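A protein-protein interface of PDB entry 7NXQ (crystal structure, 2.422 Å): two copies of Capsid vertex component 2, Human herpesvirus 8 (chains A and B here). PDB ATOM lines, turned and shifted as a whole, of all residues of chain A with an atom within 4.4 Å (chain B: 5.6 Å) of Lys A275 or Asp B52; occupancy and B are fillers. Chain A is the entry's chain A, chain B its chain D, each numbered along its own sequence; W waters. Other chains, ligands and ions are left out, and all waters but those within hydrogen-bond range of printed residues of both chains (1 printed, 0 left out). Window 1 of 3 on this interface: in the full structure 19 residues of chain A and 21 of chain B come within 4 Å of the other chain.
The side-chain carboxylate (OD2) of Asp B52 lies within salt-bridge range of the side-chain amino group (NZ) of Lys A275 (3.3 Å).
The side-chain hydroxyl (OG1) of Thr A31 sits close to the side-chain amino group (NZ) of Lys A275, 3.3 Å away. The side-chain hydroxyl of Thr B51 is in hydrogen-bond range of the backbone carbonyl oxygen of Phe B47 (2.7 Å). The side-chain amide nitrogen (NE2) of Gln B56 lies close to the backbone carbonyl oxygen (O) of Asp B52 (3.5 Å).
Thr A31 touches Asp B52 (CG2 to OD2, 3.5 Å). Gln B56 touches Thr A31. Thr B51 touches Met A34 (O to CE, 3.7 Å). Asp B52 touches Met A34. Met B55 touches Met A34. Leu A272 touches Val B342 (CD1 to CG2, 3.6 Å). Phe B341 touches Lys A275 (O to O, 3.8 Å).
Printed residues of chain B within 4 Å of Thr A31: Asp B52 and Gln B56. Lys A275 touches just these residues of chain B: Asp B52 (3.3 Å) and Phe B341 (3.8 Å). Gln A277 touches none of the printed residues of chain B. Asp B52 touches just these residues of chain A: Thr A31 (3.5 Å), Met A34 (3.2 Å) and Lys A275 (3.3 Å). Printed residues of chain A within 4 Å of Gln B56: Thr A31. Asn B343 touches none of the printed residues of chain A. The nearest residue of chain B that does not touch Lys A275 is Ser B49 (4.02 Å). The nearest printed residue of chain A that does not touch Asp B52 is Leu A272 (6.6 Å). The nearest printed residue of chain B that does not touch Thr A31 is Leu B344 (4.6 Å).
Of the 8 printed residues of chain A, 4 touch a printed residue of chain B. Printed residues of chain A that touch a printed residue of chain B: Thr A31, Met A34, Leu A272 and Lys A275. Of the 14 printed residues of chain B, 6 touch a printed residue of chain A. Printed residues of chain B that touch a printed residue of chain A: Thr B51, Asp B52, Met B55, Gln B56, Phe B341 and Val B342. Hydrophobic or aromatic side chains of chain B that line the printed part of chain A: Met B55 and Val B342.
No position is printed for both chains.
Water W1 lies within hydrogen-bond range of the backbone carbonyl oxygen of Thr A31 (2.7 Å), the side-chain carboxylate of Asp B52 (2.7 Å) and the side-chain amino group of Lys A275 (3.1 Å).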
ATOM      1  N   THR A  31     -14.567  11.438 -20.630  1.00  0.00           N
ATOM      2  CA  THR A  31     -15.388  10.797 -19.601  1.00  0.00           C
ATOM      3  C   THR A  31     -15.355  11.531 -18.254  1.00  0.00           C
ATOM      4  O   THR A  31     -16.184  11.248 -17.400  1.00  0.00           O
ATOM      5  CB  THR A  31     -15.023   9.316 -19.451  1.00  0.00           C
ATOM      6  OG1 THR A  31     -13.792   9.178 -18.738  1.00  0.00           O
ATOM      7  CG2 THR A  31     -14.956   8.585 -20.786  1.00  0.00           C
ATOM      8  N   MET A  34     -18.605  14.358 -17.459  1.00  0.00           N
ATOM      9  CA  MET A  34     -19.951  13.808 -17.518  1.00  0.00           C
ATOM     10  C   MET A  34     -20.715  13.856 -16.195  1.00  0.00           C
ATOM     11  O   MET A  34     -21.800  13.282 -16.095  1.00  0.00           O
ATOM     12  CB  MET A  34     -19.882  12.364 -18.035  1.00  0.00           C
ATOM     13  CG  MET A  34     -19.076  12.215 -19.310  1.00  0.00           C
ATOM     14  SD  MET A  34     -19.941  12.946 -20.716  1.00  0.00           S
ATOM     15  CE  MET A  34     -21.295  11.829 -20.888  1.00  0.00           C
ATOM     16  N   LEU A 272     -12.990   6.974 -12.612  1.00  0.00           N
ATOM     17  CA  LEU A 272     -13.804   6.077 -13.423  1.00  0.00           C
ATOM     18  C   LEU A 272     -15.149   5.720 -12.831  1.00  0.00           C
ATOM     19  O   LEU A 272     -16.108   5.556 -13.582  1.00  0.00           O
ATOM     20  CB  LEU A 272     -13.025   4.799 -13.771  1.00  0.00           C
ATOM     21  CG  LEU A 272     -11.653   5.024 -14.396  1.00  0.00           C
ATOM     22  CD1 LEU A 272     -10.869   3.745 -14.468  1.00  0.00           C
ATOM     23  CD2 LEU A 272     -11.768   5.678 -15.750  1.00  0.00           C
ATOM     24  N   GLY A 273     -15.220   5.575 -11.517  1.00  0.00           N
ATOM     25  CA  GLY A 273     -16.477   5.238 -10.859  1.00  0.00           C
ATOM     26  C   GLY A 273     -17.038   3.885 -11.253  1.00  0.00           C
ATOM     27  O   GLY A 273     -16.343   2.872 -11.138  1.00  0.00           O
ATOM     28  N   PRO A 274     -18.290   3.849 -11.768  1.00  0.00           N
ATOM     29  CA  PRO A 274     -18.912   2.562 -12.145  1.00  0.00           C
ATOM     30  C   PRO A 274     -18.274   1.825 -13.324  1.00  0.00           C
ATOM     31  O   PRO A 274     -18.551   0.638 -13.519  1.00  0.00           O
ATOM     32  CB  PRO A 274     -20.373   2.931 -12.442  1.00  0.00           C
ATOM     33  CG  PRO A 274     -20.565   4.292 -11.866  1.00  0.00           C
ATOM     34  CD  PRO A 274     -19.226   4.967 -11.960  1.00  0.00           C
ATOM     35  N   LYS A 275     -17.437   2.517 -14.113  1.00  0.00           N
ATOM     36  CA  LYS A 275     -16.733   1.904 -15.242  1.00  0.00           C
ATOM     37  C   LYS A 275     -15.638   0.925 -14.756  1.00  0.00           C
ATOM     38  O   LYS A 275     -15.320  -0.047 -15.446  1.00  0.00           O
ATOM     39  CB  LYS A 275     -16.124   2.989 -16.146  1.00  0.00           C
ATOM     40  CG  LYS A 275     -17.075   3.519 -17.209  1.00  0.00           C
ATOM     41  CD  LYS A 275     -16.575   4.832 -17.790  1.00  0.00           C
ATOM     42  CE  LYS A 275     -16.757   5.966 -16.815  1.00  0.00           C
ATOM     43  NZ  LYS A 275     -15.875   7.120 -17.139  1.00  0.00           N
ATOM     44  N   PHE A 276     -15.075   1.185 -13.565  1.00  0.00           N
ATOM     45  CA  PHE A 276     -14.031   0.380 -12.951  1.00  0.00           C
ATOM     46  C   PHE A 276     -14.656  -0.707 -12.052  1.00  0.00           C
ATOM     47  O   PHE A 276     -15.405  -0.393 -11.130  1.00  0.00           O
ATOM     48  CB  PHE A 276     -13.130   1.311 -12.108  1.00  0.00           C
ATOM     49  CG  PHE A 276     -11.827   0.763 -11.568  1.00  0.00           C
ATOM     50  CD1 PHE A 276     -11.495  -0.571 -11.725  1.00  0.00           C
ATOM     51  CD2 PHE A 276     -10.931   1.588 -10.909  1.00  0.00           C
ATOM     52  CE1 PHE A 276     -10.309  -1.073 -11.215  1.00  0.00           C
ATOM     53  CE2 PHE A 276      -9.738   1.086 -10.412  1.00  0.00           C
ATOM     54  CZ  PHE A 276      -9.443  -0.245 -10.554  1.00  0.00           C
ATOM     55  N   GLN A 277     -14.330  -1.980 -12.311  1.00  0.00           N
ATOM     56  CA  GLN A 277     -14.737  -3.103 -11.462  1.00  0.00           C
ATOM     57  C   GLN A 277     -13.476  -3.464 -10.642  1.00  0.00           C
ATOM     58  O   GLN A 277     -12.566  -4.095 -11.184  1.00  0.00           O
ATOM     59  CB  GLN A 277     -15.182  -4.296 -12.318  1.00  0.00           C
ATOM     60  CG  GLN A 277     -16.647  -4.204 -12.745  1.00  0.00           C
ATOM     61  CD  GLN A 277     -17.376  -5.517 -12.539  1.00  0.00           C
ATOM     62  OE1 GLN A 277     -16.899  -6.592 -12.923  1.00  0.00           O
ATOM     63  NE2 GLN A 277     -18.551  -5.459 -11.926  1.00  0.00           N
ATOM     64  N   PHE B  47     -25.430   2.022 -19.901  1.00  0.00           N
ATOM     65  CA  PHE B  47     -25.947   3.291 -20.408  1.00  0.00           C
ATOM     66  C   PHE B  47     -25.038   4.473 -20.070  1.00  0.00           C
ATOM     67  O   PHE B  47     -25.001   5.439 -20.825  1.00  0.00           O
ATOM     68  CB  PHE B  47     -27.390   3.529 -19.975  1.00  0.00           C
ATOM     69  CG  PHE B  47     -28.369   2.598 -20.649  1.00  0.00           C
ATOM     70  CD1 PHE B  47     -28.867   2.884 -21.911  1.00  0.00           C
ATOM     71  CD2 PHE B  47     -28.783   1.431 -20.026  1.00  0.00           C
ATOM     72  CE1 PHE B  47     -29.766   2.025 -22.533  1.00  0.00           C
ATOM     73  CE2 PHE B  47     -29.675   0.569 -20.654  1.00  0.00           C
ATOM     74  CZ  PHE B  47     -30.166   0.875 -21.900  1.00  0.00           C
ATOM     75  N   ILE B  48     -24.273   4.390 -18.975  1.00  0.00           N
ATOM     76  CA  ILE B  48     -23.288   5.409 -18.621  1.00  0.00           C
ATOM     77  C   ILE B  48     -22.162   5.364 -19.663  1.00  0.00           C
ATOM     78  O   ILE B  48     -21.733   6.413 -20.136  1.00  0.00           O
ATOM     79  CB  ILE B  48     -22.752   5.175 -17.180  1.00  0.00           C
ATOM     80  CG1 ILE B  48     -23.841   5.471 -16.129  1.00  0.00           C
ATOM     81  CG2 ILE B  48     -21.490   5.986 -16.904  1.00  0.00           C
ATOM     82  CD1 ILE B  48     -23.520   4.980 -14.765  1.00  0.00           C
ATOM     83  N   SER B  49     -21.723   4.151 -20.055  1.00  0.00           N
ATOM     84  CA  SER B  49     -20.695   3.948 -21.081  1.00  0.00           C
ATOM     85  C   SER B  49     -21.216   4.395 -22.451  1.00  0.00           C
ATOM     86  O   SER B  49     -20.461   4.969 -23.235  1.00  0.00           O
ATOM     87  CB  SER B  49     -20.287   2.479 -21.157  1.00  0.00           C
ATOM     88  OG  SER B  49     -19.589   2.073 -19.993  1.00  0.00           O
ATOM     89  N   LEU B  50     -22.499   4.124 -22.742  1.00  0.00           N
ATOM     90  CA  LEU B  50     -23.152   4.523 -23.982  1.00  0.00           C
ATOM     91  C   LEU B  50     -23.170   6.041 -24.064  1.00  0.00           C
ATOM     92  O   LEU B  50     -22.847   6.582 -25.108  1.00  0.00           O
ATOM     93  CB  LEU B  50     -24.595   3.969 -24.038  1.00  0.00           C
ATOM     94  CG  LEU B  50     -25.412   4.299 -25.297  1.00  0.00           C
ATOM     95  CD1 LEU B  50     -26.331   3.155 -25.658  1.00  0.00           C
ATOM     96  CD2 LEU B  50     -26.226   5.577 -25.138  1.00  0.00           C
ATOM     97  N   THR B  51     -23.535   6.725 -22.968  1.00  0.00           N
ATOM     98  CA  THR B  51     -23.614   8.180 -22.915  1.00  0.00           C
ATOM     99  C   THR B  51     -22.241   8.781 -23.101  1.00  0.00           C
ATOM    100  O   THR B  51     -22.097   9.717 -23.875  1.00  0.00           O
ATOM    101  CB  THR B  51     -24.322   8.638 -21.632  1.00  0.00           C
ATOM    102  OG1 THR B  51     -25.569   7.959 -21.520  1.00  0.00           O
ATOM    103  CG2 THR B  51     -24.566  10.122 -21.610  1.00  0.00           C
ATOM    104  N   ASP B  52     -21.215   8.205 -22.453  1.00  0.00           N
ATOM    105  CA  ASP B  52     -19.821   8.637 -22.601  1.00  0.00           C
ATOM    106  C   ASP B  52     -19.388   8.545 -24.062  1.00  0.00           C
ATOM    107  O   ASP B  52     -18.775   9.477 -24.582  1.00  0.00           O
ATOM    108  CB  ASP B  52     -18.875   7.729 -21.783  1.00  0.00           C
ATOM    109  CG  ASP B  52     -18.735   8.072 -20.322  1.00  0.00           C
ATOM    110  OD1 ASP B  52     -19.328   9.082 -19.892  1.00  0.00           O
ATOM    111  OD2 ASP B  52     -18.031   7.323 -19.601  1.00  0.00           O
ATOM    112  N   ASN B  53     -19.693   7.416 -24.718  1.00  0.00           N
ATOM    113  CA  ASN B  53     -19.319   7.174 -26.103  1.00  0.00           C
ATOM    114  C   ASN B  53     -20.069   8.064 -27.070  1.00  0.00           C
ATOM    115  O   ASN B  53     -19.448   8.635 -27.948  1.00  0.00           O
ATOM    116  CB  ASN B  53     -19.525   5.713 -26.469  1.00  0.00           C
ATOM    117  CG  ASN B  53     -18.730   5.316 -27.679  1.00  0.00           C
ATOM    118  OD1 ASN B  53     -19.290   5.020 -28.736  1.00  0.00           O
ATOM    119  ND2 ASN B  53     -17.408   5.318 -27.547  1.00  0.00           N
ATOM    120  N   ALA B  54     -21.386   8.223 -26.890  1.00  0.00           N
ATOM    121  CA  ALA B  54     -22.222   9.056 -27.740  1.00  0.00           C
ATOM    122  C   ALA B  54     -21.742  10.496 -27.793  1.00  0.00           C
ATOM    123  O   ALA B  54     -21.746  11.091 -28.863  1.00  0.00           O
ATOM    124  CB  ALA B  54     -23.655   9.012 -27.248  1.00  0.00           C
ATOM    125  N   MET B  55     -21.303  11.061 -26.652  1.00  0.00           N
ATOM    126  CA  MET B  55     -20.829  12.444 -26.608  1.00  0.00           C
ATOM    127  C   MET B  55     -19.469  12.639 -27.284  1.00  0.00           C
ATOM    128  O   MET B  55     -19.136  13.763 -27.656  1.00  0.00           O
ATOM    129  CB  MET B  55     -20.827  12.999 -25.169  1.00  0.00           C
ATOM    130  CG  MET B  55     -22.190  12.928 -24.473  1.00  0.00           C
ATOM    131  SD  MET B  55     -23.556  13.772 -25.328  1.00  0.00           S
ATOM    132  CE  MET B  55     -24.518  12.401 -25.887  1.00  0.00           C
ATOM    133  N   GLN B  56     -18.691  11.552 -27.457  1.00  0.00           N
ATOM    134  CA  GLN B  56     -17.375  11.571 -28.107  1.00  0.00           C
ATOM    135  C   GLN B  56     -17.465  11.350 -29.619  1.00  0.00           C
ATOM    136  O   GLN B  56     -16.531  11.696 -30.329  1.00  0.00           O
ATOM    137  CB  GLN B  56     -16.471  10.473 -27.528  1.00  0.00           C
ATOM    138  CG  GLN B  56     -16.042  10.683 -26.094  1.00  0.00           C
ATOM    139  CD  GLN B  56     -15.173   9.550 -25.604  1.00  0.00           C
ATOM    140  OE1 GLN B  56     -14.376   8.977 -26.349  1.00  0.00           O
ATOM    141  NE2 GLN B  56     -15.303   9.204 -24.338  1.00  0.00           N
ATOM    142  N   PHE B 341     -11.008  -4.591 -15.618  1.00  0.00           N
ATOM    143  CA  PHE B 341     -10.952  -4.033 -16.960  1.00  0.00           C
ATOM    144  C   PHE B 341     -11.909  -2.848 -17.151  1.00  0.00           C
ATOM    145  O   PHE B 341     -13.046  -2.876 -16.689  1.00  0.00           O
ATOM    146  CB  PHE B 341     -11.175  -5.178 -17.960  1.00  0.00           C
ATOM    147  CG  PHE B 341     -12.042  -4.990 -19.174  1.00  0.00           C
ATOM    148  CD1 PHE B 341     -13.410  -5.115 -19.086  1.00  0.00           C
ATOM    149  CD2 PHE B 341     -11.482  -4.870 -20.431  1.00  0.00           C
ATOM    150  CE1 PHE B 341     -14.210  -4.997 -20.212  1.00  0.00           C
ATOM    151  CE2 PHE B 341     -12.287  -4.769 -21.561  1.00  0.00           C
ATOM    152  CZ  PHE B 341     -13.645  -4.834 -21.446  1.00  0.00           C
ATOM    153  N   VAL B 342     -11.413  -1.788 -17.794  1.00  0.00           N
ATOM    154  CA  VAL B 342     -12.155  -0.573 -18.095  1.00  0.00           C
ATOM    155  C   VAL B 342     -12.431  -0.577 -19.588  1.00  0.00           C
ATOM    156  O   VAL B 342     -11.495  -0.567 -20.377  1.00  0.00           O
ATOM    157  CB  VAL B 342     -11.343   0.681 -17.711  1.00  0.00           C
ATOM    158  CG1 VAL B 342     -12.150   1.945 -17.947  1.00  0.00           C
ATOM    159  CG2 VAL B 342     -10.849   0.605 -16.273  1.00  0.00           C
ATOM    160  N   ASN B 343     -13.698  -0.596 -19.984  1.00  0.00           N
ATOM    161  CA  ASN B 343     -14.071  -0.633 -21.389  1.00  0.00           C
ATOM    162  C   ASN B 343     -14.381   0.756 -21.964  1.00  0.00           C
ATOM    163  O   ASN B 343     -15.471   1.277 -21.768  1.00  0.00           O
ATOM    164  CB  ASN B 343     -15.252  -1.571 -21.585  1.00  0.00           C
ATOM    165  CG  ASN B 343     -15.456  -2.028 -22.994  1.00  0.00           C
ATOM    166  OD1 ASN B 343     -14.803  -1.567 -23.926  1.00  0.00           O
ATOM    167  ND2 ASN B 343     -16.372  -2.956 -23.183  1.00  0.00           N
ATOM    168  N   LEU B 344     -13.430   1.333 -22.711  1.00  0.00           N
ATOM    169  CA  LEU B 344     -13.610   2.628 -23.373  1.00  0.00           C
ATOM    170  C   LEU B 344     -13.884   2.478 -24.889  1.00  0.00           C
ATOM    171  O   LEU B 344     -13.703   3.441 -25.640  1.00  0.00           O
ATOM    172  CB  LEU B 344     -12.374   3.520 -23.165  1.00  0.00           C
ATOM    173  CG  LEU B 344     -11.924   3.732 -21.736  1.00  0.00           C
ATOM    174  CD1 LEU B 344     -10.619   4.500 -21.685  1.00  0.00           C
ATOM    175  CD2 LEU B 344     -12.996   4.432 -20.930  1.00  0.00           C
HETATM  176  O   HOH W   1     -18.091   9.304 -17.456  1.00  0.00           O
